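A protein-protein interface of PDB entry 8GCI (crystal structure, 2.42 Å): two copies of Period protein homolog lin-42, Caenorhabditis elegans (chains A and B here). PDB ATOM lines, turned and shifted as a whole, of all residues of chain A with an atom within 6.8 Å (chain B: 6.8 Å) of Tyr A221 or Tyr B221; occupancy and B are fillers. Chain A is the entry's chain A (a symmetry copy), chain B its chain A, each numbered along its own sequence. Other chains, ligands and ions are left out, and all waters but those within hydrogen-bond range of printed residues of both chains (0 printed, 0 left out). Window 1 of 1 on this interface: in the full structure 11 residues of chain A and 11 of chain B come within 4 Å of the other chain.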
ATOM      1  N   LYS A 139       0.562  26.224   0.772  1.00  0.00           N
ATOM      2  CA  LYS A 139      -0.748  25.955   1.357  1.00  0.00           C
ATOM      3  C   LYS A 139      -1.768  25.724   0.255  1.00  0.00           C
ATOM      4  O   LYS A 139      -1.726  26.383  -0.789  1.00  0.00           O
ATOM      5  CB  LYS A 139      -1.250  27.116   2.254  1.00  0.00           C
ATOM      6  CG  LYS A 139      -0.355  27.428   3.436  1.00  0.00           C
ATOM      7  CD  LYS A 139      -0.997  28.414   4.420  1.00  0.00           C
ATOM      8  CE  LYS A 139       0.001  28.782   5.510  1.00  0.00           C
ATOM      9  NZ  LYS A 139      -0.573  29.622   6.611  1.00  0.00           N
ATOM     10  N   ARG A 192      -5.292  13.351  11.842  1.00  0.00           N
ATOM     11  CA  ARG A 192      -6.162  14.481  12.183  1.00  0.00           C
ATOM     12  C   ARG A 192      -5.414  15.811  12.079  1.00  0.00           C
ATOM     13  O   ARG A 192      -5.684  16.752  12.829  1.00  0.00           O
ATOM     14  CB  ARG A 192      -6.791  14.312  13.578  1.00  0.00           C
ATOM     15  CG  ARG A 192      -7.447  12.937  13.822  1.00  0.00           C
ATOM     16  CD  ARG A 192      -7.512  12.542  15.307  1.00  0.00           C
ATOM     17  NE  ARG A 192      -8.438  13.355  16.091  1.00  0.00           N
ATOM     18  CZ  ARG A 192      -8.081  14.151  17.098  1.00  0.00           C
ATOM     19  NH1 ARG A 192      -6.816  14.271  17.474  1.00  0.00           N
ATOM     20  NH2 ARG A 192      -9.018  14.839  17.747  1.00  0.00           N
ATOM     21  N   GLY A 193      -4.456  15.904  11.153  1.00  0.00           N
ATOM     22  CA  GLY A 193      -3.780  17.156  10.875  1.00  0.00           C
ATOM     23  C   GLY A 193      -2.426  17.344  11.535  1.00  0.00           C
ATOM     24  O   GLY A 193      -1.703  18.277  11.156  1.00  0.00           O
ATOM     25  N   TRP A 218       4.229  17.677   6.529  1.00  0.00           N
ATOM     26  CA  TRP A 218       2.865  18.065   6.200  1.00  0.00           C
ATOM     27  C   TRP A 218       2.063  18.335   7.463  1.00  0.00           C
ATOM     28  O   TRP A 218       2.231  17.657   8.483  1.00  0.00           O
ATOM     29  CB  TRP A 218       2.161  16.992   5.348  1.00  0.00           C
ATOM     30  CG  TRP A 218       2.929  16.633   4.116  1.00  0.00           C
ATOM     31  CD1 TRP A 218       4.029  15.833   4.045  1.00  0.00           C
ATOM     32  CD2 TRP A 218       2.676  17.096   2.779  1.00  0.00           C
ATOM     33  NE1 TRP A 218       4.467  15.759   2.751  1.00  0.00           N
ATOM     34  CE2 TRP A 218       3.660  16.527   1.953  1.00  0.00           C
ATOM     35  CE3 TRP A 218       1.716  17.939   2.206  1.00  0.00           C
ATOM     36  CZ2 TRP A 218       3.712  16.761   0.572  1.00  0.00           C
ATOM     37  CZ3 TRP A 218       1.758  18.169   0.834  1.00  0.00           C
ATOM     38  CH2 TRP A 218       2.751  17.581   0.032  1.00  0.00           C
ATOM     39  N   SER A 219       1.196  19.341   7.378  1.00  0.00           N
ATOM     40  CA  SER A 219       0.258  19.683   8.434  1.00  0.00           C
ATOM     41  C   SER A 219      -1.091  19.976   7.786  1.00  0.00           C
ATOM     42  O   SER A 219      -1.167  20.307   6.598  1.00  0.00           O
ATOM     43  CB  SER A 219       0.768  20.879   9.262  1.00  0.00           C
ATOM     44  OG  SER A 219      -0.138  21.263  10.292  1.00  0.00           O
ATOM     45  N   ALA A 220      -2.163  19.854   8.577  1.00  0.00           N
ATOM     46  CA  ALA A 220      -3.515  20.035   8.060  1.00  0.00           C
ATOM     47  C   ALA A 220      -4.435  20.619   9.133  1.00  0.00           C
ATOM     48  O   ALA A 220      -4.352  20.240  10.303  1.00  0.00           O
ATOM     49  CB  ALA A 220      -4.086  18.703   7.565  1.00  0.00           C
ATOM     50  N   TYR A 221      -5.315  21.534   8.727  1.00  0.00           N
ATOM     51  CA  TYR A 221      -6.330  22.076   9.619  1.00  0.00           C
ATOM     52  C   TYR A 221      -7.625  21.309   9.424  1.00  0.00           C
ATOM     53  O   TYR A 221      -8.120  21.189   8.295  1.00  0.00           O
ATOM     54  CB  TYR A 221      -6.572  23.566   9.363  1.00  0.00           C
ATOM     55  CG  TYR A 221      -7.815  24.094  10.056  1.00  0.00           C
ATOM     56  CD1 TYR A 221      -7.830  24.313  11.433  1.00  0.00           C
ATOM     57  CD2 TYR A 221      -8.982  24.369   9.335  1.00  0.00           C
ATOM     58  CE1 TYR A 221      -8.967  24.797  12.072  1.00  0.00           C
ATOM     59  CE2 TYR A 221     -10.125  24.848   9.965  1.00  0.00           C
ATOM     60  CZ  TYR A 221     -10.113  25.061  11.329  1.00  0.00           C
ATOM     61  OH  TYR A 221     -11.243  25.539  11.960  1.00  0.00           O
ATOM     62  N   VAL A 222      -8.173  20.787  10.517  1.00  0.00           N
ATOM     63  CA  VAL A 222      -9.448  20.080  10.482  1.00  0.00           C
ATOM     64  C   VAL A 222     -10.517  20.982  11.081  1.00  0.00           C
ATOM     65  O   VAL A 222     -10.445  21.355  12.261  1.00  0.00           O
ATOM     66  CB  VAL A 222      -9.383  18.731  11.210  1.00  0.00           C
ATOM     67  CG1 VAL A 222     -10.732  18.022  11.103  1.00  0.00           C
ATOM     68  CG2 VAL A 222      -8.291  17.854  10.601  1.00  0.00           C
ATOM     69  N   ASN A 223     -11.499  21.341  10.267  1.00  0.00           N
ATOM     70  CA  ASN A 223     -12.659  22.092  10.745  1.00  0.00           C
ATOM     71  C   ASN A 223     -13.349  21.278  11.827  1.00  0.00           C
ATOM     72  O   ASN A 223     -13.758  20.142  11.564  1.00  0.00           O
ATOM     73  CB  ASN A 223     -13.615  22.380   9.588  1.00  0.00           C
ATOM     74  CG  ASN A 223     -14.810  23.211   9.997  1.00  0.00           C
ATOM     75  OD1 ASN A 223     -15.571  22.826  10.883  1.00  0.00           O
ATOM     76  ND2 ASN A 223     -15.006  24.342   9.324  1.00  0.00           N
ATOM     77  N   PRO A 224     -13.490  21.796  13.042  1.00  0.00           N
ATOM     78  CA  PRO A 224     -14.093  20.985  14.112  1.00  0.00           C
ATOM     79  C   PRO A 224     -15.601  20.740  13.960  1.00  0.00           C
ATOM     80  O   PRO A 224     -16.115  19.808  14.595  1.00  0.00           O
ATOM     81  CB  PRO A 224     -13.777  21.790  15.374  1.00  0.00           C
ATOM     82  CG  PRO A 224     -13.681  23.212  14.888  1.00  0.00           C
ATOM     83  CD  PRO A 224     -13.084  23.134  13.504  1.00  0.00           C
ATOM     84  N   TRP A 225     -16.322  21.509  13.135  1.00  0.00           N
ATOM     85  CA  TRP A 225     -17.765  21.309  12.960  1.00  0.00           C
ATOM     86  C   TRP A 225     -18.088  20.328  11.837  1.00  0.00           C
ATOM     87  O   TRP A 225     -18.943  19.456  12.006  1.00  0.00           O
ATOM     88  CB  TRP A 225     -18.468  22.651  12.706  1.00  0.00           C
ATOM     89  CG  TRP A 225     -18.217  23.621  13.812  1.00  0.00           C
ATOM     90  CD1 TRP A 225     -18.813  23.637  15.050  1.00  0.00           C
ATOM     91  CD2 TRP A 225     -17.270  24.699  13.809  1.00  0.00           C
ATOM     92  NE1 TRP A 225     -18.291  24.653  15.809  1.00  0.00           N
ATOM     93  CE2 TRP A 225     -17.348  25.325  15.072  1.00  0.00           C
ATOM     94  CE3 TRP A 225     -16.369  25.202  12.859  1.00  0.00           C
ATOM     95  CZ2 TRP A 225     -16.556  26.421  15.407  1.00  0.00           C
ATOM     96  CZ3 TRP A 225     -15.598  26.295  13.196  1.00  0.00           C
ATOM     97  CH2 TRP A 225     -15.692  26.891  14.459  1.00  0.00           C
ATOM     98  N   LYS A 228     -13.794  17.882   8.633  1.00  0.00           N
ATOM     99  CA  LYS A 228     -13.033  17.635   7.417  1.00  0.00           C
ATOM    100  C   LYS A 228     -11.790  18.522   7.342  1.00  0.00           C
ATOM    101  O   LYS A 228     -11.759  19.638   7.876  1.00  0.00           O
ATOM    102  CB  LYS A 228     -13.923  17.847   6.190  1.00  0.00           C
ATOM    103  CG  LYS A 228     -15.123  16.887   6.176  1.00  0.00           C
ATOM    104  CD  LYS A 228     -16.097  17.241   5.094  1.00  0.00           C
ATOM    105  CE  LYS A 228     -17.225  16.211   4.997  1.00  0.00           C
ATOM    106  NZ  LYS A 228     -18.082  16.564   3.844  1.00  0.00           N
ATOM    107  N   MET A 229     -10.756  18.003   6.687  1.00  0.00           N
ATOM    108  CA  MET A 229      -9.580  18.811   6.406  1.00  0.00           C
ATOM    109  C   MET A 229      -9.970  19.955   5.490  1.00  0.00           C
ATOM    110  O   MET A 229     -10.625  19.740   4.465  1.00  0.00           O
ATOM    111  CB  MET A 229      -8.492  17.964   5.741  1.00  0.00           C
ATOM    112  CG  MET A 229      -8.108  16.710   6.519  1.00  0.00           C
ATOM    113  SD  MET A 229      -7.074  15.576   5.554  1.00  0.00           S
ATOM    114  CE  MET A 229      -5.984  16.727   4.709  1.00  0.00           C
ATOM    115  N   GLU A 230      -9.569  21.179   5.849  1.00  0.00           N
ATOM    116  CA  GLU A 230      -9.863  22.319   4.991  1.00  0.00           C
ATOM    117  C   GLU A 230      -8.636  23.119   4.612  1.00  0.00           C
ATOM    118  O   GLU A 230      -8.750  24.042   3.799  1.00  0.00           O
ATOM    119  CB  GLU A 230     -10.898  23.262   5.649  1.00  0.00           C
ATOM    120  CG  GLU A 230     -12.269  22.612   5.881  1.00  0.00           C
ATOM    121  CD  GLU A 230     -13.374  23.609   6.252  1.00  0.00           C
ATOM    122  OE1 GLU A 230     -13.072  24.784   6.548  1.00  0.00           O
ATOM    123  OE2 GLU A 230     -14.556  23.210   6.228  1.00  0.00           O
ATOM    124  N   LEU A 231      -7.479  22.823   5.188  1.00  0.00           N
ATOM    125  CA  LEU A 231      -6.240  23.447   4.756  1.00  0.00           C
ATOM    126  C   LEU A 231      -5.145  22.415   4.916  1.00  0.00           C
ATOM    127  O   LEU A 231      -5.092  21.707   5.929  1.00  0.00           O
ATOM    128  CB  LEU A 231      -5.910  24.714   5.557  1.00  0.00           C
ATOM    129  CG  LEU A 231      -4.685  25.529   5.128  1.00  0.00           C
ATOM    130  CD1 LEU A 231      -4.969  26.279   3.826  1.00  0.00           C
ATOM    131  CD2 LEU A 231      -4.302  26.508   6.227  1.00  0.00           C
ATOM    132  N   VAL A 232      -4.301  22.305   3.899  1.00  0.00           N
ATOM    133  CA  VAL A 232      -3.115  21.468   3.961  1.00  0.00           C
ATOM    134  C   VAL A 232      -1.908  22.373   3.815  1.00  0.00           C
ATOM    135  O   VAL A 232      -1.824  23.157   2.859  1.00  0.00           O
ATOM    136  CB  VAL A 232      -3.117  20.378   2.872  1.00  0.00           C
ATOM    137  CG1 VAL A 232      -1.836  19.605   2.929  1.00  0.00           C
ATOM    138  CG2 VAL A 232      -4.337  19.454   3.056  1.00  0.00           C
ATOM    139  N   VAL A 233      -0.983  22.263   4.766  1.00  0.00           N
ATOM    140  CA  VAL A 233       0.223  23.075   4.819  1.00  0.00           C
ATOM    141  C   VAL A 233       1.417  22.145   4.686  1.00  0.00           C
ATOM    142  O   VAL A 233       1.482  21.108   5.357  1.00  0.00           O
ATOM    143  CB  VAL A 233       0.309  23.873   6.136  1.00  0.00           C
ATOM    144  CG1 VAL A 233       1.503  24.841   6.115  1.00  0.00           C
ATOM    145  CG2 VAL A 233      -0.972  24.615   6.389  1.00  0.00           C
ATOM    146  N   ALA A 234       2.372  22.533   3.854  1.00  0.00           N
ATOM    147  CA  ALA A 234       3.555  21.723   3.596  1.00  0.00           C
ATOM    148  C   ALA A 234       4.783  22.599   3.780  1.00  0.00           C
ATOM    149  O   ALA A 234       4.835  23.715   3.248  1.00  0.00           O
ATOM    150  CB  ALA A 234       3.507  21.121   2.183  1.00  0.00           C
ATOM    151  N   LYS B 139     -13.551  33.367   7.788  1.00  0.00           N
ATOM    152  CA  LYS B 139     -12.155  33.009   8.016  1.00  0.00           C
ATOM    153  C   LYS B 139     -11.271  34.230   7.835  1.00  0.00           C
ATOM    154  O   LYS B 139     -11.517  35.060   6.952  1.00  0.00           O
ATOM    155  CB  LYS B 139     -11.660  31.898   7.052  1.00  0.00           C
ATOM    156  CG  LYS B 139     -12.419  30.591   7.159  1.00  0.00           C
ATOM    157  CD  LYS B 139     -11.756  29.456   6.367  1.00  0.00           C
ATOM    158  CE  LYS B 139     -12.633  28.212   6.411  1.00  0.00           C
ATOM    159  NZ  LYS B 139     -12.008  26.997   5.796  1.00  0.00           N
ATOM    160  N   ARG B 192      -5.006  26.646  22.082  1.00  0.00           N
ATOM    161  CA  ARG B 192      -4.219  26.115  20.965  1.00  0.00           C
ATOM    162  C   ARG B 192      -5.106  25.796  19.760  1.00  0.00           C
ATOM    163  O   ARG B 192      -4.836  24.861  19.003  1.00  0.00           O
ATOM    164  CB  ARG B 192      -3.397  24.883  21.384  1.00  0.00           C
ATOM    165  CG  ARG B 192      -2.578  25.070  22.678  1.00  0.00           C
ATOM    166  CD  ARG B 192      -2.278  23.752  23.411  1.00  0.00           C
ATOM    167  NE  ARG B 192      -1.344  22.882  22.699  1.00  0.00           N
ATOM    168  CZ  ARG B 192      -1.644  21.674  22.227  1.00  0.00           C
ATOM    169  NH1 ARG B 192      -2.855  21.153  22.370  1.00  0.00           N
ATOM    170  NH2 ARG B 192      -0.705  20.969  21.600  1.00  0.00           N
ATOM    171  N   GLY B 193      -6.182  26.564  19.571  1.00  0.00           N
ATOM    172  CA  GLY B 193      -7.012  26.440  18.390  1.00  0.00           C
ATOM    173  C   GLY B 193      -8.280  25.619  18.549  1.00  0.00           C
ATOM    174  O   GLY B 193      -9.138  25.669  17.655  1.00  0.00           O
ATOM    175  N   TRP B 218     -15.536  29.665  17.887  1.00  0.00           N
ATOM    176  CA  TRP B 218     -14.274  30.021  17.254  1.00  0.00           C
ATOM    177  C   TRP B 218     -13.344  28.819  17.196  1.00  0.00           C
ATOM    178  O   TRP B 218     -13.306  27.996  18.118  1.00  0.00           O
ATOM    179  CB  TRP B 218     -13.583  31.187  17.984  1.00  0.00           C
ATOM    180  CG  TRP B 218     -14.466  32.385  18.129  1.00  0.00           C
ATOM    181  CD1 TRP B 218     -15.479  32.548  19.027  1.00  0.00           C
ATOM    182  CD2 TRP B 218     -14.441  33.576  17.326  1.00  0.00           C
ATOM    183  NE1 TRP B 218     -16.074  33.765  18.840  1.00  0.00           N
ATOM    184  CE2 TRP B 218     -15.462  34.416  17.801  1.00  0.00           C
ATOM    185  CE3 TRP B 218     -13.656  34.007  16.249  1.00  0.00           C
ATOM    186  CZ2 TRP B 218     -15.719  35.678  17.246  1.00  0.00           C
ATOM    187  CZ3 TRP B 218     -13.902  35.262  15.699  1.00  0.00           C
ATOM    188  CH2 TRP B 218     -14.926  36.083  16.200  1.00  0.00           C
ATOM    189  N   SER B 219     -12.603  28.730  16.095  1.00  0.00           N
ATOM    190  CA  SER B 219     -11.574  27.723  15.900  1.00  0.00           C
ATOM    191  C   SER B 219     -10.359  28.407  15.282  1.00  0.00           C
ATOM    192  O   SER B 219     -10.475  29.470  14.664  1.00  0.00           O
ATOM    193  CB  SER B 219     -12.089  26.567  15.020  1.00  0.00           C
ATOM    194  OG  SER B 219     -11.099  25.570  14.782  1.00  0.00           O
ATOM    195  N   ALA B 220      -9.186  27.788  15.451  1.00  0.00           N
ATOM    196  CA  ALA B 220      -7.939  28.376  14.973  1.00  0.00           C
ATOM    197  C   ALA B 220      -6.950  27.288  14.552  1.00  0.00           C
ATOM    198  O   ALA B 220      -6.838  26.253  15.212  1.00  0.00           O
ATOM    199  CB  ALA B 220      -7.305  29.253  16.056  1.00  0.00           C
ATOM    200  N   TYR B 221      -6.229  27.532  13.457  1.00  0.00           N
ATOM    201  CA  TYR B 221      -5.166  26.638  13.020  1.00  0.00           C
ATOM    202  C   TYR B 221      -3.836  27.155  13.539  1.00  0.00           C
ATOM    203  O   TYR B 221      -3.485  28.322  13.313  1.00  0.00           O
ATOM    204  CB  TYR B 221      -5.112  26.525  11.494  1.00  0.00           C
ATOM    205  CG  TYR B 221      -3.849  25.850  10.991  1.00  0.00           C
ATOM    206  CD1 TYR B 221      -3.675  24.472  11.115  1.00  0.00           C
ATOM    207  CD2 TYR B 221      -2.822  26.591  10.398  1.00  0.00           C
ATOM    208  CE1 TYR B 221      -2.519  23.849  10.656  1.00  0.00           C
ATOM    209  CE2 TYR B 221      -1.661  25.979   9.940  1.00  0.00           C
ATOM    210  CZ  TYR B 221      -1.514  24.612  10.069  1.00  0.00           C
ATOM    211  OH  TYR B 221      -0.366  23.998   9.615  1.00  0.00           O
ATOM    212  N   VAL B 222      -3.099  26.295  14.234  1.00  0.00           N
ATOM    213  CA  VAL B 222      -1.774  26.642  14.737  1.00  0.00           C
ATOM    214  C   VAL B 222      -0.732  25.942  13.875  1.00  0.00           C
ATOM    215  O   VAL B 222      -0.686  24.705  13.814  1.00  0.00           O
ATOM    216  CB  VAL B 222      -1.605  26.283  16.219  1.00  0.00           C
ATOM    217  CG1 VAL B 222      -0.216  26.707  16.696  1.00  0.00           C
ATOM    218  CG2 VAL B 222      -2.672  26.983  17.057  1.00  0.00           C
ATOM    219  N   ASN B 223       0.092  26.732  13.202  1.00  0.00           N
ATOM    220  CA  ASN B 223       1.221  26.198  12.444  1.00  0.00           C
ATOM    221  C   ASN B 223       2.128  25.438  13.399  1.00  0.00           C
ATOM    222  O   ASN B 223       2.612  26.025  14.372  1.00  0.00           O
ATOM    223  CB  ASN B 223       1.982  27.333  11.759  1.00  0.00           C
ATOM    224  CG  ASN B 223       3.130  26.847  10.903  1.00  0.00           C
ATOM    225  OD1 ASN B 223       4.036  26.173  11.388  1.00  0.00           O
ATOM    226  ND2 ASN B 223       3.119  27.222   9.627  1.00  0.00           N
ATOM    227  N   PRO B 224       2.374  24.151  13.179  1.00  0.00           N
ATOM    228  CA  PRO B 224       3.193  23.394  14.139  1.00  0.00           C
ATOM    229  C   PRO B 224       4.684  23.757  14.139  1.00  0.00           C
ATOM    230  O   PRO B 224       5.370  23.439  15.121  1.00  0.00           O
ATOM    231  CB  PRO B 224       2.965  21.942  13.715  1.00  0.00           C
ATOM    232  CG  PRO B 224       2.662  22.032  12.243  1.00  0.00           C
ATOM    233  CD  PRO B 224       1.899  23.321  12.060  1.00  0.00           C
ATOM    234  N   TRP B 225       5.209  24.425  13.104  1.00  0.00           N
ATOM    235  CA  TRP B 225       6.629  24.792  13.063  1.00  0.00           C
ATOM    236  C   TRP B 225       6.899  26.156  13.689  1.00  0.00           C
ATOM    237  O   TRP B 225       7.853  26.306  14.455  1.00  0.00           O
ATOM    238  CB  TRP B 225       7.151  24.761  11.618  1.00  0.00           C
ATOM    239  CG  TRP B 225       6.950  23.423  10.989  1.00  0.00           C
ATOM    240  CD1 TRP B 225       7.700  22.291  11.197  1.00  0.00           C
ATOM    241  CD2 TRP B 225       5.907  23.052  10.078  1.00  0.00           C
ATOM    242  NE1 TRP B 225       7.182  21.246  10.475  1.00  0.00           N
ATOM    243  CE2 TRP B 225       6.086  21.685   9.774  1.00  0.00           C
ATOM    244  CE3 TRP B 225       4.842  23.743   9.482  1.00  0.00           C
ATOM    245  CZ2 TRP B 225       5.238  20.999   8.907  1.00  0.00           C
ATOM    246  CZ3 TRP B 225       4.014  23.059   8.616  1.00  0.00           C
ATOM    247  CH2 TRP B 225       4.214  21.701   8.338  1.00  0.00           C
ATOM    248  N   LYS B 228       2.492  29.428  15.825  1.00  0.00           N
ATOM    249  CA  LYS B 228       1.606  30.582  15.866  1.00  0.00           C
ATOM    250  C   LYS B 228       0.280  30.299  15.159  1.00  0.00           C
ATOM    251  O   LYS B 228       0.206  29.495  14.221  1.00  0.00           O
ATOM    252  CB  LYS B 228       2.300  31.797  15.246  1.00  0.00           C
ATOM    253  CG  LYS B 228       3.579  32.180  16.006  1.00  0.00           C
ATOM    254  CD  LYS B 228       4.361  33.228  15.274  1.00  0.00           C
ATOM    255  CE  LYS B 228       5.565  33.702  16.091  1.00  0.00           C
ATOM    256  NZ  LYS B 228       6.221  34.806  15.358  1.00  0.00           N
ATOM    257  N   MET B 229      -0.773  30.957  15.635  1.00  0.00           N
ATOM    258  CA  MET B 229      -2.052  30.899  14.945  1.00  0.00           C
ATOM    259  C   MET B 229      -1.905  31.524  13.571  1.00  0.00           C
ATOM    260  O   MET B 229      -1.372  32.630  13.441  1.00  0.00           O
ATOM    261  CB  MET B 229      -3.127  31.645  15.741  1.00  0.00           C
ATOM    262  CG  MET B 229      -3.275  31.182  17.186  1.00  0.00           C
ATOM    263  SD  MET B 229      -4.306  32.296  18.176  1.00  0.00           S
ATOM    264  CE  MET B 229      -5.609  32.700  17.008  1.00  0.00           C
ATOM    265  N   GLU B 230      -2.378  30.822  12.536  1.00  0.00           N
ATOM    266  CA  GLU B 230      -2.317  31.383  11.192  1.00  0.00           C
ATOM    267  C   GLU B 230      -3.659  31.415  10.493  1.00  0.00           C
ATOM    268  O   GLU B 230      -3.748  31.970   9.393  1.00  0.00           O
ATOM    269  CB  GLU B 230      -1.307  30.613  10.310  1.00  0.00           C
ATOM    270  CG  GLU B 230       0.143  30.698  10.810  1.00  0.00           C
ATOM    271  CD  GLU B 230       1.180  30.196   9.797  1.00  0.00           C
ATOM    272  OE1 GLU B 230       0.800  29.578   8.780  1.00  0.00           O
ATOM    273  OE2 GLU B 230       2.383  30.443  10.018  1.00  0.00           O
ATOM    274  N   LEU B 231      -4.693  30.820  11.070  1.00  0.00           N
ATOM    275  CA  LEU B 231      -6.036  30.948  10.529  1.00  0.00           C
ATOM    276  C   LEU B 231      -6.989  30.949  11.705  1.00  0.00           C
ATOM    277  O   LEU B 231      -6.835  30.153  12.638  1.00  0.00           O
ATOM    278  CB  LEU B 231      -6.385  29.818   9.551  1.00  0.00           C
ATOM    279  CG  LEU B 231      -7.732  29.895   8.824  1.00  0.00           C
ATOM    280  CD1 LEU B 231      -7.700  30.982   7.750  1.00  0.00           C
ATOM    281  CD2 LEU B 231      -8.065  28.548   8.203  1.00  0.00           C
ATOM    282  N   VAL B 232      -7.944  31.868  11.673  1.00  0.00           N
ATOM    283  CA  VAL B 232      -9.020  31.904  12.649  1.00  0.00           C
ATOM    284  C   VAL B 232     -10.322  31.688  11.904  1.00  0.00           C
ATOM    285  O   VAL B 232     -10.611  32.396  10.928  1.00  0.00           O
ATOM    286  CB  VAL B 232      -9.051  33.231  13.431  1.00  0.00           C
ATOM    287  CG1 VAL B 232     -10.227  33.246  14.356  1.00  0.00           C
ATOM    288  CG2 VAL B 232      -7.729  33.417  14.202  1.00  0.00           C
ATOM    289  N   VAL B 233     -11.097  30.708  12.363  1.00  0.00           N
ATOM    290  CA  VAL B 233     -12.362  30.325  11.754  1.00  0.00           C
ATOM    291  C   VAL B 233     -13.462  30.571  12.773  1.00  0.00           C
ATOM    292  O   VAL B 233     -13.332  30.187  13.942  1.00  0.00           O
ATOM    293  CB  VAL B 233     -12.355  28.845  11.321  1.00  0.00           C
ATOM    294  CG1 VAL B 233     -13.633  28.495  10.543  1.00  0.00           C
ATOM    295  CG2 VAL B 233     -11.133  28.541  10.500  1.00  0.00           C
ATOM    296  N   ALA B 234     -14.553  31.173  12.324  1.00  0.00           N
ATOM    297  CA  ALA B 234     -15.670  31.509  13.195  1.00  0.00           C
ATOM    298  C   ALA B 234     -16.947  30.981  12.560  1.00  0.00           C
ATOM    299  O   ALA B 234     -17.182  31.199  11.365  1.00  0.00           O
ATOM    300  CB  ALA B 234     -15.749  33.027  13.423  1.00  0.00           C
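The side-chain amino group of Lys B139 lies within salt-bridge range of the side-chain carboxylate of Glu A230, 2.6 Å away. The side-chain hydroxyl of Ser B219 sits at hydrogen-bond distance from the side-chain hydroxyl of Tyr A221, 2.8 Å away. OH of Tyr B221 sits at hydrogen-bond distance from OG of Ser A219. The side-chain carboxylate (OE1) of Glu B230 is in salt-bridge range of the side-chain amino group (NZ) of Lys A139.
The backbone carbonyl oxygen (O) of Gly B193 is in hydrogen-bond range of the side-chain hydroxyl (OG) of Ser B219 (3.5 Å). O of Tyr B221 sits at hydrogen-bond distance from N of Glu B230 (2.8 Å). The side-chain amide oxygen (OD1) of Asn B223 lies within hydrogen-bond range of the backbone NH (N) of Trp B225, 2.7 Å away. The side-chain amide nitrogen (ND2) of Asn B223 is in hydrogen-bond range of the side-chain carboxylate (OE2) of Glu B230 (3.3 Å). The backbone carbonyl oxygen of Gly A193 sits at hydrogen-bond distance from the side-chain hydroxyl of Ser A219 (3.5 Å). N of Tyr A221 is in hydrogen-bond range of O of Leu A231 (2.8 Å).
Among the printed residues, pairs that only touch across the chains: Ser A219 with Pro B224 (3.4 Å), Ser A219 with Trp B225 (3.7 Å), Tyr A221 with Tyr B221 (3.5 Å), Tyr A221 with Val B233 (3.3 Å), Pro A224 with Ser B219 (3.4 Å), Trp A225 with Ser B219 (3.7 Å), Trp A225 with Val B233 (3.97 Å), Val A233 with Tyr B221 (3.3 Å) and Val A233 with Trp B225 (3.97 Å).
Tyr B221 touches just these residues of chain A: Ser A219 (2.8 Å), Tyr A221 (3.5 Å) and Val A233 (3.3 Å). Printed residues of chain B within 4 Å of Lys A139: Glu B230. Of the printed residues of chain A, Glu B230 touches Lys A139. Of the printed residues of chain A, Lys B139 touches Glu A230 (2.6 Å). Printed residues of chain B within 4 Å of Pro A224: Ser B219 (3.4 Å). Ala A220 touches none of the printed residues of chain B. The nearest residue of chain B that does not touch Tyr A221 is Ala B220 (4.1 Å). The nearest printed residue of chain A that does not touch Ser B219 is Val A222 (5.0 Å).
Of the 18 printed residues of chain A, 7 touch a printed residue of chain B. Hydrophobic or aromatic side chains of chain A that line the printed part of chain B: Tyr A221, Pro A224, Trp A225 and Val A233. Among the printed residues, 13 pairs touch across the chains. Among the printed residues, Asp or Glu carboxylates within 4 Å of a Lys or Arg side-chain nitrogen of the other chain: Lys A139 with Glu B230 (2.6 Å) and Glu A230 with Lys B139 (2.6 Å).
Ser A219 touches Tyr B221, and with the chains exchanged Tyr A221 touches Ser B219. Ser A219 touches Pro B224, and with the chains exchanged Pro A224 touches Ser B219. Tyr A221 touches its own counterpart, Tyr B221. Tyr A221 touches Val B233, and with the chains exchanged Val A233 touches Tyr B221. Positions printed for both chains: 139, 192, 193, 218, 219, 220, 221, 222, 223, 224, 225, 228, 229, 230, 231, 232, 233 and 234. Of the 13 pairs that touch across the chains among the printed residues, 13 have their exchanged pair printed and touching as well.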
